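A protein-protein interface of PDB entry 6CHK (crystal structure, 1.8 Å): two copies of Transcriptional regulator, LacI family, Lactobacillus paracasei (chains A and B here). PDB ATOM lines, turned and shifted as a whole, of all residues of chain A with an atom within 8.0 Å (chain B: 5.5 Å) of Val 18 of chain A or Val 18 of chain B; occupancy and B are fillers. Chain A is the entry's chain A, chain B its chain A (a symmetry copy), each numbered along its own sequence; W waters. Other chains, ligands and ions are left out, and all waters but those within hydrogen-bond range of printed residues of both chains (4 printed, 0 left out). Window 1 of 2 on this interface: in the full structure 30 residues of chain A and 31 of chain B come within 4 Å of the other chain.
The side-chain amide nitrogen (NE2) of Gln 45 of chain B lies within hydrogen-bond range of the side-chain carboxylate (OD1) of Asp 28 of chain A (2.9 Å). The side-chain carboxylate (OE1) of Glu 31 of chain A lies within hydrogen-bond range of the side-chain amide nitrogen (NE2) of Gln 45 of chain B. The backbone NH (N) of Ile 43 of chain A is in hydrogen-bond range of the backbone carbonyl oxygen (O) of Ile 43 of chain B, 3.0 Å away.
Water W4 lies within hydrogen-bond range of O of Val 41 of chain A (2.7 Å), N of Gln 45 of chain B (2.9 Å) and OE2 of Glu 31 of chain A (3.4 Å). Water W1 bridges OG1 of Thr 19 of chain B (2.7 Å) and OD2 of Asp 28 of chain A (2.7 Å). Water W2 bridges the backbone carbonyl oxygen (O) of Gln 45 of chain B (2.7 Å) and the side-chain carboxylate (OE2) of Glu 31 of chain A (2.8 Å). Water W3 lies within hydrogen-bond range of OE1 of Gln 45 of chain B, OG1 of Thr 19 of chain B, N of Val 18 of chain B and OD1 of Asp 28 of chain A.
Of the printed residues of chain B, Val 18 of chain A touches Val 18 (3.9 Å), Ala 24 (3.9 Å) and Phe 27 (3.98 Å). Printed residues of chain B within 4 Å of Phe 27 of chain A: Val 18 and Gln 45. Of the printed residues of chain A, Val 18 of chain B touches Val 18, Ala 24 and Phe 27. Of the printed residues of chain A, Ala 24 of chain B touches Val 18 (3.9 Å) and Thr 19 (3.6 Å). Printed residues of chain A within 4 Å of Ile 43 of chain B: Ile 43 (2.9 Å). The nearest printed residue of chain B that does not touch Val 18 of chain A is Ile 43 of chain B (5.4 Å). The nearest printed residue of chain A that does not touch Val 18 of chain B is Ile 43 of chain A (5.4 Å). The nearest printed residue of chain B that does not touch Ala 24 of chain A is Ala 24 of chain B (5.3 Å).
Among the printed residues, pairs that only touch across the chains: Val 18 of chain A with Val 18 of chain B (3.9 Å), Val 18 of chain A with Ala 24 of chain B (3.9 Å), Val 18 of chain A with Phe 27 of chain B (3.98 Å), Thr 19 of chain A with Ala 24 of chain B (3.6 Å), Ala 24 of chain A with Val 18 of chain B (3.9 Å), Ala 24 of chain A with Thr 19 of chain B (3.6 Å), Gly 25 of chain A with Thr 19 of chain B (3.98 Å), Phe 27 of chain A with Val 18 of chain B (3.98 Å), Phe 27 of chain A with Gln 45 of chain B (3.99 Å), Asp 28 of chain A with Thr 19 of chain B (3.6 Å), Val 41 of chain A with Thr 44 of chain B (3.9 Å) and Gln 45 of chain A with Phe 27 of chain B (3.99 Å).
Hydrophobic or aromatic side chains of chain A within 4 Å of the printed part of chain B: Val 18, Ala 24, Phe 27 and Ile 43.
Val 18 of chain B touches its own counterpart, Val 18 of chain A. Thr 19 of chain A touches Ala 24 of chain B, and with the chains exchanged Ala 24 of chain A touches Thr 19 of chain B. Phe 27 of chain A touches Gln 45 of chain B, and with the chains exchanged Gln 45 of chain A touches Phe 27 of chain B. Ile 43 of chain A touches its own counterpart, Ile 43 of chain B. Of the 15 pairs that touch across the chains among the printed residues, 10 have their exchanged pair printed and touching as well.
NH1 of Arg 17 of chain A lies within hydrogen-bond range of OG1 of Thr 19 of chain A (2.9 Å). N of Val 18 of chain A sits at hydrogen-bond distance from OE1 of Gln 45 of chain A (2.8 Å). O of Thr 44 of chain B is in hydrogen-bond range of N of Val 15 of chain B (3.0 Å). The side-chain hydroxyl (OG1) of Thr 19 of chain B sits at hydrogen-bond distance from the guanidinium group (NH1) of Arg 17 of chain B (2.9 Å).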
ATOM      1  N   VAL A  13       5.297  -8.577 -15.809  1.00  0.00           N
ATOM      2  CA  VAL A  13       4.680  -7.334 -15.354  1.00  0.00           C
ATOM      3  C   VAL A  13       5.819  -6.483 -14.743  1.00  0.00           C
ATOM      4  O   VAL A  13       6.555  -6.996 -13.924  1.00  0.00           O
ATOM      5  CB  VAL A  13       3.584  -7.583 -14.322  1.00  0.00           C
ATOM      6  CG1 VAL A  13       2.988  -6.267 -13.813  1.00  0.00           C
ATOM      7  CG2 VAL A  13       2.471  -8.388 -14.974  1.00  0.00           C
ATOM      8  N   LEU A  14       5.932  -5.243 -15.174  1.00  0.00           N
ATOM      9  CA  LEU A  14       6.983  -4.310 -14.672  1.00  0.00           C
ATOM     10  C   LEU A  14       6.362  -3.268 -13.794  1.00  0.00           C
ATOM     11  O   LEU A  14       5.441  -2.562 -14.214  1.00  0.00           O
ATOM     12  CB  LEU A  14       7.705  -3.689 -15.831  1.00  0.00           C
ATOM     13  CG  LEU A  14       9.034  -2.965 -15.528  1.00  0.00           C
ATOM     14  CD1 LEU A  14      10.045  -4.001 -15.093  1.00  0.00           C
ATOM     15  CD2 LEU A  14       9.474  -2.322 -16.817  1.00  0.00           C
ATOM     16  N   VAL A  15       6.925  -3.091 -12.582  1.00  0.00           N
ATOM     17  CA  VAL A  15       6.472  -2.092 -11.619  1.00  0.00           C
ATOM     18  C   VAL A  15       7.700  -1.361 -11.056  1.00  0.00           C
ATOM     19  O   VAL A  15       8.808  -1.871 -11.134  1.00  0.00           O
ATOM     20  CB  VAL A  15       5.643  -2.668 -10.434  1.00  0.00           C
ATOM     21  CG1 VAL A  15       4.386  -3.359 -10.939  1.00  0.00           C
ATOM     22  CG2 VAL A  15       6.466  -3.550  -9.511  1.00  0.00           C
ATOM     23  N   SER A  16       7.483  -0.203 -10.462  1.00  0.00           N
ATOM     24  CA  SER A  16       8.623   0.460  -9.816  1.00  0.00           C
ATOM     25  C   SER A  16       9.082  -0.228  -8.529  1.00  0.00           C
ATOM     26  O   SER A  16      10.266  -0.440  -8.346  1.00  0.00           O
ATOM     27  CB  SER A  16       8.360   1.958  -9.589  1.00  0.00           C
ATOM     28  OG  SER A  16       7.194   2.133  -8.865  1.00  0.00           O
ATOM     29  N   ARG A  17       8.146  -0.568  -7.653  1.00  0.00           N
ATOM     30  CA  ARG A  17       8.453  -1.101  -6.321  1.00  0.00           C
ATOM     31  C   ARG A  17       7.351  -2.061  -5.908  1.00  0.00           C
ATOM     32  O   ARG A  17       6.186  -1.656  -5.784  1.00  0.00           O
ATOM     33  CB  ARG A  17       8.530   0.011  -5.268  1.00  0.00           C
ATOM     34  CG  ARG A  17       9.890   0.408  -4.714  1.00  0.00           C
ATOM     35  CD  ARG A  17       9.806   0.827  -3.218  1.00  0.00           C
ATOM     36  NE  ARG A  17       8.743   1.813  -3.057  1.00  0.00           N
ATOM     37  CZ  ARG A  17       7.737   1.849  -2.163  1.00  0.00           C
ATOM     38  NH1 ARG A  17       7.519   0.962  -1.159  1.00  0.00           N
ATOM     39  NH2 ARG A  17       6.895   2.858  -2.285  1.00  0.00           N
ATOM     40  N   VAL A  18       7.721  -3.316  -5.611  1.00  0.00           N
ATOM     41  CA  VAL A  18       6.753  -4.349  -5.191  1.00  0.00           C
ATOM     42  C   VAL A  18       6.205  -4.113  -3.766  1.00  0.00           C
ATOM     43  O   VAL A  18       5.098  -4.597  -3.415  1.00  0.00           O
ATOM     44  CB  VAL A  18       7.373  -5.772  -5.349  1.00  0.00           C
ATOM     45  CG1 VAL A  18       6.572  -6.863  -4.658  1.00  0.00           C
ATOM     46  CG2 VAL A  18       7.482  -6.120  -6.823  1.00  0.00           C
ATOM     47  N   THR A  19       6.964  -3.428  -2.928  1.00  0.00           N
ATOM     48  CA  THR A  19       6.560  -3.156  -1.552  1.00  0.00           C
ATOM     49  C   THR A  19       5.627  -1.960  -1.497  1.00  0.00           C
ATOM     50  O   THR A  19       5.238  -1.561  -0.421  1.00  0.00           O
ATOM     51  CB  THR A  19       7.753  -2.866  -0.607  1.00  0.00           C
ATOM     52  OG1 THR A  19       8.546  -1.793  -1.148  1.00  0.00           O
ATOM     53  CG2 THR A  19       8.602  -4.138  -0.437  1.00  0.00           C
ATOM     54  N   ASN A  20       5.336  -1.351  -2.638  1.00  0.00           N
ATOM     55  CA  ASN A  20       4.250  -0.371  -2.726  1.00  0.00           C
ATOM     56  C   ASN A  20       2.982  -1.197  -2.875  1.00  0.00           C
ATOM     57  O   ASN A  20       2.794  -1.904  -3.902  1.00  0.00           O
ATOM     58  CB  ASN A  20       4.460   0.544  -3.912  1.00  0.00           C
ATOM     59  CG  ASN A  20       3.348   1.560  -4.120  1.00  0.00           C
ATOM     60  OD1 ASN A  20       2.209   1.308  -3.759  1.00  0.00           O
ATOM     61  ND2 ASN A  20       3.690   2.695  -4.783  1.00  0.00           N
ATOM     62  N   PRO A  21       2.100  -1.134  -1.869  1.00  0.00           N
ATOM     63  CA  PRO A  21       0.909  -2.020  -1.973  1.00  0.00           C
ATOM     64  C   PRO A  21      -0.014  -1.764  -3.159  1.00  0.00           C
ATOM     65  O   PRO A  21      -0.798  -2.659  -3.520  1.00  0.00           O
ATOM     66  CB  PRO A  21       0.171  -1.755  -0.677  1.00  0.00           C
ATOM     67  CG  PRO A  21       1.220  -1.290   0.261  1.00  0.00           C
ATOM     68  CD  PRO A  21       2.146  -0.480  -0.553  1.00  0.00           C
ATOM     69  N   PHE A  22       0.020  -0.581  -3.749  1.00  0.00           N
ATOM     70  CA  PHE A  22      -0.708  -0.361  -4.992  1.00  0.00           C
ATOM     71  C   PHE A  22      -0.133  -1.228  -6.132  1.00  0.00           C
ATOM     72  O   PHE A  22      -0.880  -1.865  -6.858  1.00  0.00           O
ATOM     73  CB  PHE A  22      -0.724   1.115  -5.384  1.00  0.00           C
ATOM     74  CG  PHE A  22      -1.136   1.360  -6.791  1.00  0.00           C
ATOM     75  CD1 PHE A  22      -2.478   1.291  -7.146  1.00  0.00           C
ATOM     76  CD2 PHE A  22      -0.182   1.539  -7.773  1.00  0.00           C
ATOM     77  CE1 PHE A  22      -2.864   1.473  -8.459  1.00  0.00           C
ATOM     78  CE2 PHE A  22      -0.548   1.710  -9.089  1.00  0.00           C
ATOM     79  CZ  PHE A  22      -1.904   1.677  -9.436  1.00  0.00           C
ATOM     80  N   PHE A  23       1.164  -1.256  -6.308  1.00  0.00           N
ATOM     81  CA  PHE A  23       1.728  -2.124  -7.338  1.00  0.00           C
ATOM     82  C   PHE A  23       1.538  -3.618  -7.046  1.00  0.00           C
ATOM     83  O   PHE A  23       1.316  -4.394  -7.964  1.00  0.00           O
ATOM     84  CB  PHE A  23       3.216  -1.801  -7.569  1.00  0.00           C
ATOM     85  CG  PHE A  23       3.416  -0.504  -8.293  1.00  0.00           C
ATOM     86  CD1 PHE A  23       2.826  -0.299  -9.537  1.00  0.00           C
ATOM     87  CD2 PHE A  23       4.157   0.518  -7.740  1.00  0.00           C
ATOM     88  CE1 PHE A  23       3.005   0.893 -10.215  1.00  0.00           C
ATOM     89  CE2 PHE A  23       4.275   1.752  -8.375  1.00  0.00           C
ATOM     90  CZ  PHE A  23       3.729   1.923  -9.629  1.00  0.00           C
ATOM     91  N   ALA A  24       1.655  -4.012  -5.783  1.00  0.00           N
ATOM     92  CA  ALA A  24       1.473  -5.403  -5.432  1.00  0.00           C
ATOM     93  C   ALA A  24       0.024  -5.791  -5.745  1.00  0.00           C
ATOM     94  O   ALA A  24      -0.218  -6.879  -6.309  1.00  0.00           O
ATOM     95  CB  ALA A  24       1.834  -5.650  -3.985  1.00  0.00           C
ATOM     96  N   GLY A  25      -0.937  -4.906  -5.414  1.00  0.00           N
ATOM     97  CA  GLY A  25      -2.355  -5.216  -5.711  1.00  0.00           C
ATOM     98  C   GLY A  25      -2.646  -5.313  -7.203  1.00  0.00           C
ATOM     99  O   GLY A  25      -3.448  -6.157  -7.659  1.00  0.00           O
ATOM    100  N   LEU A  26      -2.064  -4.393  -7.948  1.00  0.00           N
ATOM    101  CA  LEU A  26      -2.239  -4.362  -9.364  1.00  0.00           C
ATOM    102  C   LEU A  26      -1.698  -5.634 -10.006  1.00  0.00           C
ATOM    103  O   LEU A  26      -2.399  -6.272 -10.797  1.00  0.00           O
ATOM    104  CB  LEU A  26      -1.588  -3.131  -9.958  1.00  0.00           C
ATOM    105  CG  LEU A  26      -1.714  -3.000 -11.479  1.00  0.00           C
ATOM    106  CD1 LEU A  26      -3.167  -2.950 -11.909  1.00  0.00           C
ATOM    107  CD2 LEU A  26      -1.061  -1.695 -11.885  1.00  0.00           C
ATOM    108  N   PHE A  27      -0.505  -6.021  -9.617  1.00  0.00           N
ATOM    109  CA  PHE A  27       0.075  -7.279 -10.089  1.00  0.00           C
ATOM    110  C   PHE A  27      -0.814  -8.449  -9.734  1.00  0.00           C
ATOM    111  O   PHE A  27      -1.086  -9.351 -10.559  1.00  0.00           O
ATOM    112  CB  PHE A  27       1.420  -7.497  -9.472  1.00  0.00           C
ATOM    113  CG  PHE A  27       1.978  -8.875  -9.739  1.00  0.00           C
ATOM    114  CD1 PHE A  27       2.416  -9.242 -11.002  1.00  0.00           C
ATOM    115  CD2 PHE A  27       1.948  -9.832  -8.759  1.00  0.00           C
ATOM    116  CE1 PHE A  27       2.892 -10.530 -11.258  1.00  0.00           C
ATOM    117  CE2 PHE A  27       2.415 -11.116  -9.004  1.00  0.00           C
ATOM    118  CZ  PHE A  27       2.895 -11.445 -10.248  1.00  0.00           C
ATOM    119  N   ASP A  28      -1.249  -8.472  -8.483  1.00  0.00           N
ATOM    120  CA  ASP A  28      -2.061  -9.621  -8.050  1.00  0.00           C
ATOM    121  C   ASP A  28      -3.331  -9.758  -8.906  1.00  0.00           C
ATOM    122  O   ASP A  28      -3.747 -10.863  -9.277  1.00  0.00           O
ATOM    123  CB  ASP A  28      -2.392  -9.452  -6.583  1.00  0.00           C
ATOM    124  CG  ASP A  28      -3.262 -10.548  -6.040  1.00  0.00           C
ATOM    125  OD1 ASP A  28      -2.797 -11.705  -6.027  1.00  0.00           O
ATOM    126  OD2 ASP A  28      -4.377 -10.244  -5.506  1.00  0.00           O
ATOM    127  N   GLU A  31      -2.390 -10.998 -12.342  1.00  0.00           N
ATOM    128  CA  GLU A  31      -1.892 -12.360 -12.261  1.00  0.00           C
ATOM    129  C   GLU A  31      -3.005 -13.364 -12.069  1.00  0.00           C
ATOM    130  O   GLU A  31      -2.983 -14.397 -12.733  1.00  0.00           O
ATOM    131  CB  GLU A  31      -0.858 -12.526 -11.155  1.00  0.00           C
ATOM    132  CG  GLU A  31      -0.113 -13.869 -11.183  1.00  0.00           C
ATOM    133  CD  GLU A  31      -0.837 -14.992 -10.475  1.00  0.00           C
ATOM    134  OE1 GLU A  31      -1.621 -14.725  -9.531  1.00  0.00           O
ATOM    135  OE2 GLU A  31      -0.527 -16.165 -10.784  1.00  0.00           O
ATOM    136  N   VAL A  41       2.796 -15.770 -14.679  1.00  0.00           N
ATOM    137  CA  VAL A  41       3.035 -14.314 -14.696  1.00  0.00           C
ATOM    138  C   VAL A  41       4.113 -14.018 -13.647  1.00  0.00           C
ATOM    139  O   VAL A  41       4.083 -14.547 -12.544  1.00  0.00           O
ATOM    140  CB  VAL A  41       1.771 -13.515 -14.390  1.00  0.00           C
ATOM    141  CG1 VAL A  41       1.981 -12.045 -14.697  1.00  0.00           C
ATOM    142  CG2 VAL A  41       0.615 -14.049 -15.236  1.00  0.00           C
ATOM    143  N   ILE A  43       6.716 -10.832 -11.863  1.00  0.00           N
ATOM    144  CA  ILE A  43       6.839  -9.394 -11.691  1.00  0.00           C
ATOM    145  C   ILE A  43       8.321  -9.071 -11.543  1.00  0.00           C
ATOM    146  O   ILE A  43       9.047  -9.847 -10.915  1.00  0.00           O
ATOM    147  CB  ILE A  43       6.052  -8.876 -10.474  1.00  0.00           C
ATOM    148  CG1 ILE A  43       5.751  -7.398 -10.635  1.00  0.00           C
ATOM    149  CG2 ILE A  43       6.813  -9.029  -9.178  1.00  0.00           C
ATOM    150  CD1 ILE A  43       4.922  -6.808  -9.541  1.00  0.00           C
ATOM    151  N   THR A  44       8.701  -7.967 -12.146  1.00  0.00           N
ATOM    152  CA  THR A  44      10.048  -7.363 -12.010  1.00  0.00           C
ATOM    153  C   THR A  44       9.856  -5.936 -11.501  1.00  0.00           C
ATOM    154  O   THR A  44       8.883  -5.282 -11.842  1.00  0.00           O
ATOM    155  CB  THR A  44      10.713  -7.381 -13.363  1.00  0.00           C
ATOM    156  OG1 THR A  44      10.959  -8.760 -13.705  1.00  0.00           O
ATOM    157  CG2 THR A  44      12.033  -6.597 -13.362  1.00  0.00           C
ATOM    158  N   GLN A  45      10.763  -5.490 -10.629  1.00  0.00           N
ATOM    159  CA  GLN A  45      10.720  -4.120 -10.131  1.00  0.00           C
ATOM    160  C   GLN A  45      11.933  -3.335 -10.640  1.00  0.00           C
ATOM    161  O   GLN A  45      12.996  -3.911 -10.836  1.00  0.00           O
ATOM    162  CB  GLN A  45      10.603  -4.084  -8.624  1.00  0.00           C
ATOM    163  CG  GLN A  45      11.732  -4.694  -7.822  1.00  0.00           C
ATOM    164  CD  GLN A  45      11.491  -4.562  -6.316  1.00  0.00           C
ATOM    165  OE1 GLN A  45      10.442  -4.081  -5.882  1.00  0.00           O
ATOM    166  NE2 GLN A  45      12.487  -4.916  -5.525  1.00  0.00           N
ATOM    167  N   THR A  46      11.732  -2.040 -10.901  1.00  0.00           N
ATOM    168  CA  THR A  46      12.776  -1.217 -11.506  1.00  0.00           C
ATOM    169  C   THR A  46      13.462  -0.264 -10.572  1.00  0.00           C
ATOM    170  O   THR A  46      14.616   0.138 -10.881  1.00  0.00           O
ATOM    171  CB  THR A  46      12.227  -0.337 -12.651  1.00  0.00           C
ATOM    172  OG1 THR A  46      11.236   0.556 -12.122  1.00  0.00           O
ATOM    173  CG2 THR A  46      11.689  -1.195 -13.740  1.00  0.00           C
ATOM    174  N   TYR A  47      12.760   0.142  -9.499  1.00  0.00           N
ATOM    175  CA  TYR A  47      13.116   1.305  -8.671  1.00  0.00           C
ATOM    176  C   TYR A  47      13.441   2.510  -9.582  1.00  0.00           C
ATOM    177  O   TYR A  47      14.436   3.224  -9.363  1.00  0.00           O
ATOM    178  CB  TYR A  47      14.320   0.966  -7.779  1.00  0.00           C
ATOM    179  CG  TYR A  47      13.964   0.355  -6.460  1.00  0.00           C
ATOM    180  CD1 TYR A  47      13.665  -1.002  -6.351  1.00  0.00           C
ATOM    181  CD2 TYR A  47      13.934   1.134  -5.293  1.00  0.00           C
ATOM    182  CE1 TYR A  47      13.259  -1.542  -5.128  1.00  0.00           C
ATOM    183  CE2 TYR A  47      13.609   0.588  -4.066  1.00  0.00           C
ATOM    184  CZ  TYR A  47      13.275  -0.765  -3.987  1.00  0.00           C
ATOM    185  OH  TYR A  47      12.950  -1.273  -2.771  1.00  0.00           O
ATOM    186  N   GLU A 200       1.153   5.285   1.594  1.00  0.00           N
ATOM    187  CA  GLU A 200       2.326   4.936   2.399  1.00  0.00           C
ATOM    188  C   GLU A 200       2.896   6.164   3.064  1.00  0.00           C
ATOM    189  O   GLU A 200       3.099   6.147   4.276  1.00  0.00           O
ATOM    190  CB  GLU A 200       3.449   4.252   1.575  1.00  0.00           C
ATOM    191  CG  GLU A 200       3.103   2.879   0.971  1.00  0.00           C
ATOM    192  CD  GLU A 200       4.265   2.351   0.104  1.00  0.00           C
ATOM    193  OE1 GLU A 200       4.317   2.723  -1.094  1.00  0.00           O
ATOM    194  OE2 GLU A 200       5.147   1.611   0.641  1.00  0.00           O
ATOM    195  N   VAL B  15       6.782 -17.225  -3.936  1.00  0.00           N
ATOM    196  CA  VAL B  15       6.085 -16.869  -2.703  1.00  0.00           C
ATOM    197  C   VAL B  15       4.622 -17.323  -2.818  1.00  0.00           C
ATOM    198  O   VAL B  15       4.130 -17.538  -3.916  1.00  0.00           O
ATOM    199  CB  VAL B  15       6.114 -15.351  -2.361  1.00  0.00           C
ATOM    200  CG1 VAL B  15       7.544 -14.862  -2.187  1.00  0.00           C
ATOM    201  CG2 VAL B  15       5.324 -14.507  -3.348  1.00  0.00           C
ATOM    202  N   SER B  16       3.939 -17.421  -1.693  1.00  0.00           N
ATOM    203  CA  SER B  16       2.510 -17.742  -1.786  1.00  0.00           C
ATOM    204  C   SER B  16       1.657 -16.590  -2.322  1.00  0.00           C
ATOM    205  O   SER B  16       0.832 -16.801  -3.190  1.00  0.00           O
ATOM    206  CB  SER B  16       1.956 -18.279  -0.456  1.00  0.00           C
ATOM    207  OG  SER B  16       2.209 -17.378   0.564  1.00  0.00           O
ATOM    208  N   ARG B  17       1.860 -15.388  -1.800  1.00  0.00           N
ATOM    209  CA  ARG B  17       1.020 -14.227  -2.115  1.00  0.00           C
ATOM    210  C   ARG B  17       1.871 -12.970  -2.047  1.00  0.00           C
ATOM    211  O   ARG B  17       2.412 -12.641  -0.981  1.00  0.00           O
ATOM    212  CB  ARG B  17      -0.132 -14.072  -1.114  1.00  0.00           C
ATOM    213  CG  ARG B  17      -1.547 -14.405  -1.564  1.00  0.00           C
ATOM    214  CD  ARG B  17      -2.601 -13.483  -0.886  1.00  0.00           C
ATOM    215  NE  ARG B  17      -2.378 -13.480   0.554  1.00  0.00           N
ATOM    216  CZ  ARG B  17      -2.285 -12.440   1.404  1.00  0.00           C
ATOM    217  NH1 ARG B  17      -2.429 -11.127   1.090  1.00  0.00           N
ATOM    218  NH2 ARG B  17      -2.039 -12.746   2.664  1.00  0.00           N
ATOM    219  N   VAL B  18       1.925 -12.216  -3.155  1.00  0.00           N
ATOM    220  CA  VAL B  18       2.710 -10.967  -3.225  1.00  0.00           C
ATOM    221  C   VAL B  18       2.082  -9.818  -2.405  1.00  0.00           C
ATOM    222  O   VAL B  18       2.789  -8.863  -1.993  1.00  0.00           O
ATOM    223  CB  VAL B  18       2.951 -10.558  -4.712  1.00  0.00           C
ATOM    224  CG1 VAL B  18       3.475  -9.142  -4.875  1.00  0.00           C
ATOM    225  CG2 VAL B  18       3.947 -11.512  -5.347  1.00  0.00           C
ATOM    226  N   THR B  19       0.777  -9.859  -2.200  1.00  0.00           N
ATOM    227  CA  THR B  19       0.070  -8.822  -1.455  1.00  0.00           C
ATOM    228  C   THR B  19       0.192  -9.062   0.039  1.00  0.00           C
ATOM    229  O   THR B  19      -0.386  -8.323   0.807  1.00  0.00           O
ATOM    230  CB  THR B  19      -1.439  -8.740  -1.798  1.00  0.00           C
ATOM    231  OG1 THR B  19      -2.046 -10.032  -1.612  1.00  0.00           O
ATOM    232  CG2 THR B  19      -1.617  -8.259  -3.248  1.00  0.00           C
ATOM    233  N   ASN B  20       0.870 -10.128   0.439  1.00  0.00           N
ATOM    234  CA  ASN B  20       1.269 -10.298   1.840  1.00  0.00           C
ATOM    235  C   ASN B  20       2.534  -9.469   1.995  1.00  0.00           C
ATOM    236  O   ASN B  20       3.586  -9.779   1.372  1.00  0.00           O
ATOM    237  CB  ASN B  20       1.522 -11.759   2.141  1.00  0.00           C
ATOM    238  CG  ASN B  20       2.000 -12.028   3.560  1.00  0.00           C
ATOM    239  OD1 ASN B  20       2.631 -11.178   4.168  1.00  0.00           O
ATOM    240  ND2 ASN B  20       1.748 -13.269   4.051  1.00  0.00           N
ATOM    241  N   PRO B  21       2.462  -8.408   2.810  1.00  0.00           N
ATOM    242  CA  PRO B  21       3.670  -7.542   2.881  1.00  0.00           C
ATOM    243  C   PRO B  21       4.937  -8.204   3.408  1.00  0.00           C
ATOM    244  O   PRO B  21       6.040  -7.684   3.163  1.00  0.00           O
ATOM    245  CB  PRO B  21       3.240  -6.431   3.815  1.00  0.00           C
ATOM    246  CG  PRO B  21       1.763  -6.392   3.694  1.00  0.00           C
ATOM    247  CD  PRO B  21       1.343  -7.798   3.542  1.00  0.00           C
ATOM    248  N   PHE B  23       5.945 -11.287   2.386  1.00  0.00           N
ATOM    249  CA  PHE B  23       6.559 -11.806   1.167  1.00  0.00           C
ATOM    250  C   PHE B  23       7.084 -10.708   0.235  1.00  0.00           C
ATOM    251  O   PHE B  23       8.118 -10.887  -0.395  1.00  0.00           O
ATOM    252  CB  PHE B  23       5.585 -12.734   0.418  1.00  0.00           C
ATOM    253  CG  PHE B  23       5.403 -14.052   1.108  1.00  0.00           C
ATOM    254  CD1 PHE B  23       6.505 -14.860   1.375  1.00  0.00           C
ATOM    255  CD2 PHE B  23       4.157 -14.480   1.516  1.00  0.00           C
ATOM    256  CE1 PHE B  23       6.348 -16.079   2.010  1.00  0.00           C
ATOM    257  CE2 PHE B  23       3.999 -15.666   2.229  1.00  0.00           C
ATOM    258  CZ  PHE B  23       5.091 -16.481   2.441  1.00  0.00           C
ATOM    259  N   ALA B  24       6.361  -9.599   0.130  1.00  0.00           N
ATOM    260  CA  ALA B  24       6.804  -8.516  -0.718  1.00  0.00           C
ATOM    261  C   ALA B  24       8.122  -7.973  -0.157  1.00  0.00           C
ATOM    262  O   ALA B  24       9.066  -7.712  -0.931  1.00  0.00           O
ATOM    263  CB  ALA B  24       5.743  -7.444  -0.830  1.00  0.00           C
ATOM    264  N   PHE B  27      11.016 -10.530  -0.800  1.00  0.00           N
ATOM    265  CA  PHE B  27      11.419 -10.429  -2.203  1.00  0.00           C
ATOM    266  C   PHE B  27      12.246  -9.186  -2.439  1.00  0.00           C
ATOM    267  O   PHE B  27      13.301  -9.207  -3.111  1.00  0.00           O
ATOM    268  CB  PHE B  27      10.214 -10.376  -3.089  1.00  0.00           C
ATOM    269  CG  PHE B  27      10.548 -10.049  -4.525  1.00  0.00           C
ATOM    270  CD1 PHE B  27      11.199 -10.964  -5.339  1.00  0.00           C
ATOM    271  CD2 PHE B  27      10.322  -8.791  -5.015  1.00  0.00           C
ATOM    272  CE1 PHE B  27      11.545 -10.645  -6.654  1.00  0.00           C
ATOM    273  CE2 PHE B  27      10.666  -8.462  -6.319  1.00  0.00           C
ATOM    274  CZ  PHE B  27      11.262  -9.400  -7.128  1.00  0.00           C
ATOM    275  N   ILE B  43       9.490 -12.428  -9.426  1.00  0.00           N
ATOM    276  CA  ILE B  43       8.737 -13.123  -8.395  1.00  0.00           C
ATOM    277  C   ILE B  43       7.527 -13.767  -9.061  1.00  0.00           C
ATOM    278  O   ILE B  43       6.947 -13.163  -9.969  1.00  0.00           O
ATOM    279  CB  ILE B  43       8.291 -12.189  -7.257  1.00  0.00           C
ATOM    280  CG1 ILE B  43       8.016 -12.988  -5.998  1.00  0.00           C
ATOM    281  CG2 ILE B  43       7.022 -11.437  -7.583  1.00  0.00           C
ATOM    282  CD1 ILE B  43       7.648 -12.167  -4.806  1.00  0.00           C
ATOM    283  N   THR B  44       7.223 -14.960  -8.605  1.00  0.00           N
ATOM    284  CA  THR B  44       6.001 -15.712  -8.978  1.00  0.00           C
ATOM    285  C   THR B  44       5.249 -16.027  -7.687  1.00  0.00           C
ATOM    286  O   THR B  44       5.861 -16.255  -6.655  1.00  0.00           O
ATOM    287  CB  THR B  44       6.420 -16.971  -9.695  1.00  0.00           C
ATOM    288  OG1 THR B  44       7.010 -16.577 -10.950  1.00  0.00           O
ATOM    289  CG2 THR B  44       5.231 -17.909  -9.945  1.00  0.00           C
ATOM    290  N   GLN B  45       3.917 -15.971  -7.746  1.00  0.00           N
ATOM    291  CA  GLN B  45       3.096 -16.323  -6.595  1.00  0.00           C
ATOM    292  C   GLN B  45       2.300 -17.600  -6.883  1.00  0.00           C
ATOM    293  O   GLN B  45       1.939 -17.851  -8.026  1.00  0.00           O
ATOM    294  CB  GLN B  45       2.206 -15.173  -6.178  1.00  0.00           C
ATOM    295  CG  GLN B  45       1.182 -14.686  -7.181  1.00  0.00           C
ATOM    296  CD  GLN B  45       0.338 -13.542  -6.617  1.00  0.00           C
ATOM    297  OE1 GLN B  45       0.577 -13.068  -5.504  1.00  0.00           O
ATOM    298  NE2 GLN B  45      -0.690 -13.149  -7.346  1.00  0.00           N
HETATM  299  O   HOH W   1      -4.485 -10.422  -2.765  1.00  0.00           O
HETATM  300  O   HOH W   2      -0.002 -18.726  -9.734  1.00  0.00           O
HETATM  301  O   HOH W   3      -1.036 -11.909  -3.531  1.00  0.00           O
HETATM  302  O   HOH W   4       2.761 -15.358 -10.337  1.00  0.00           O
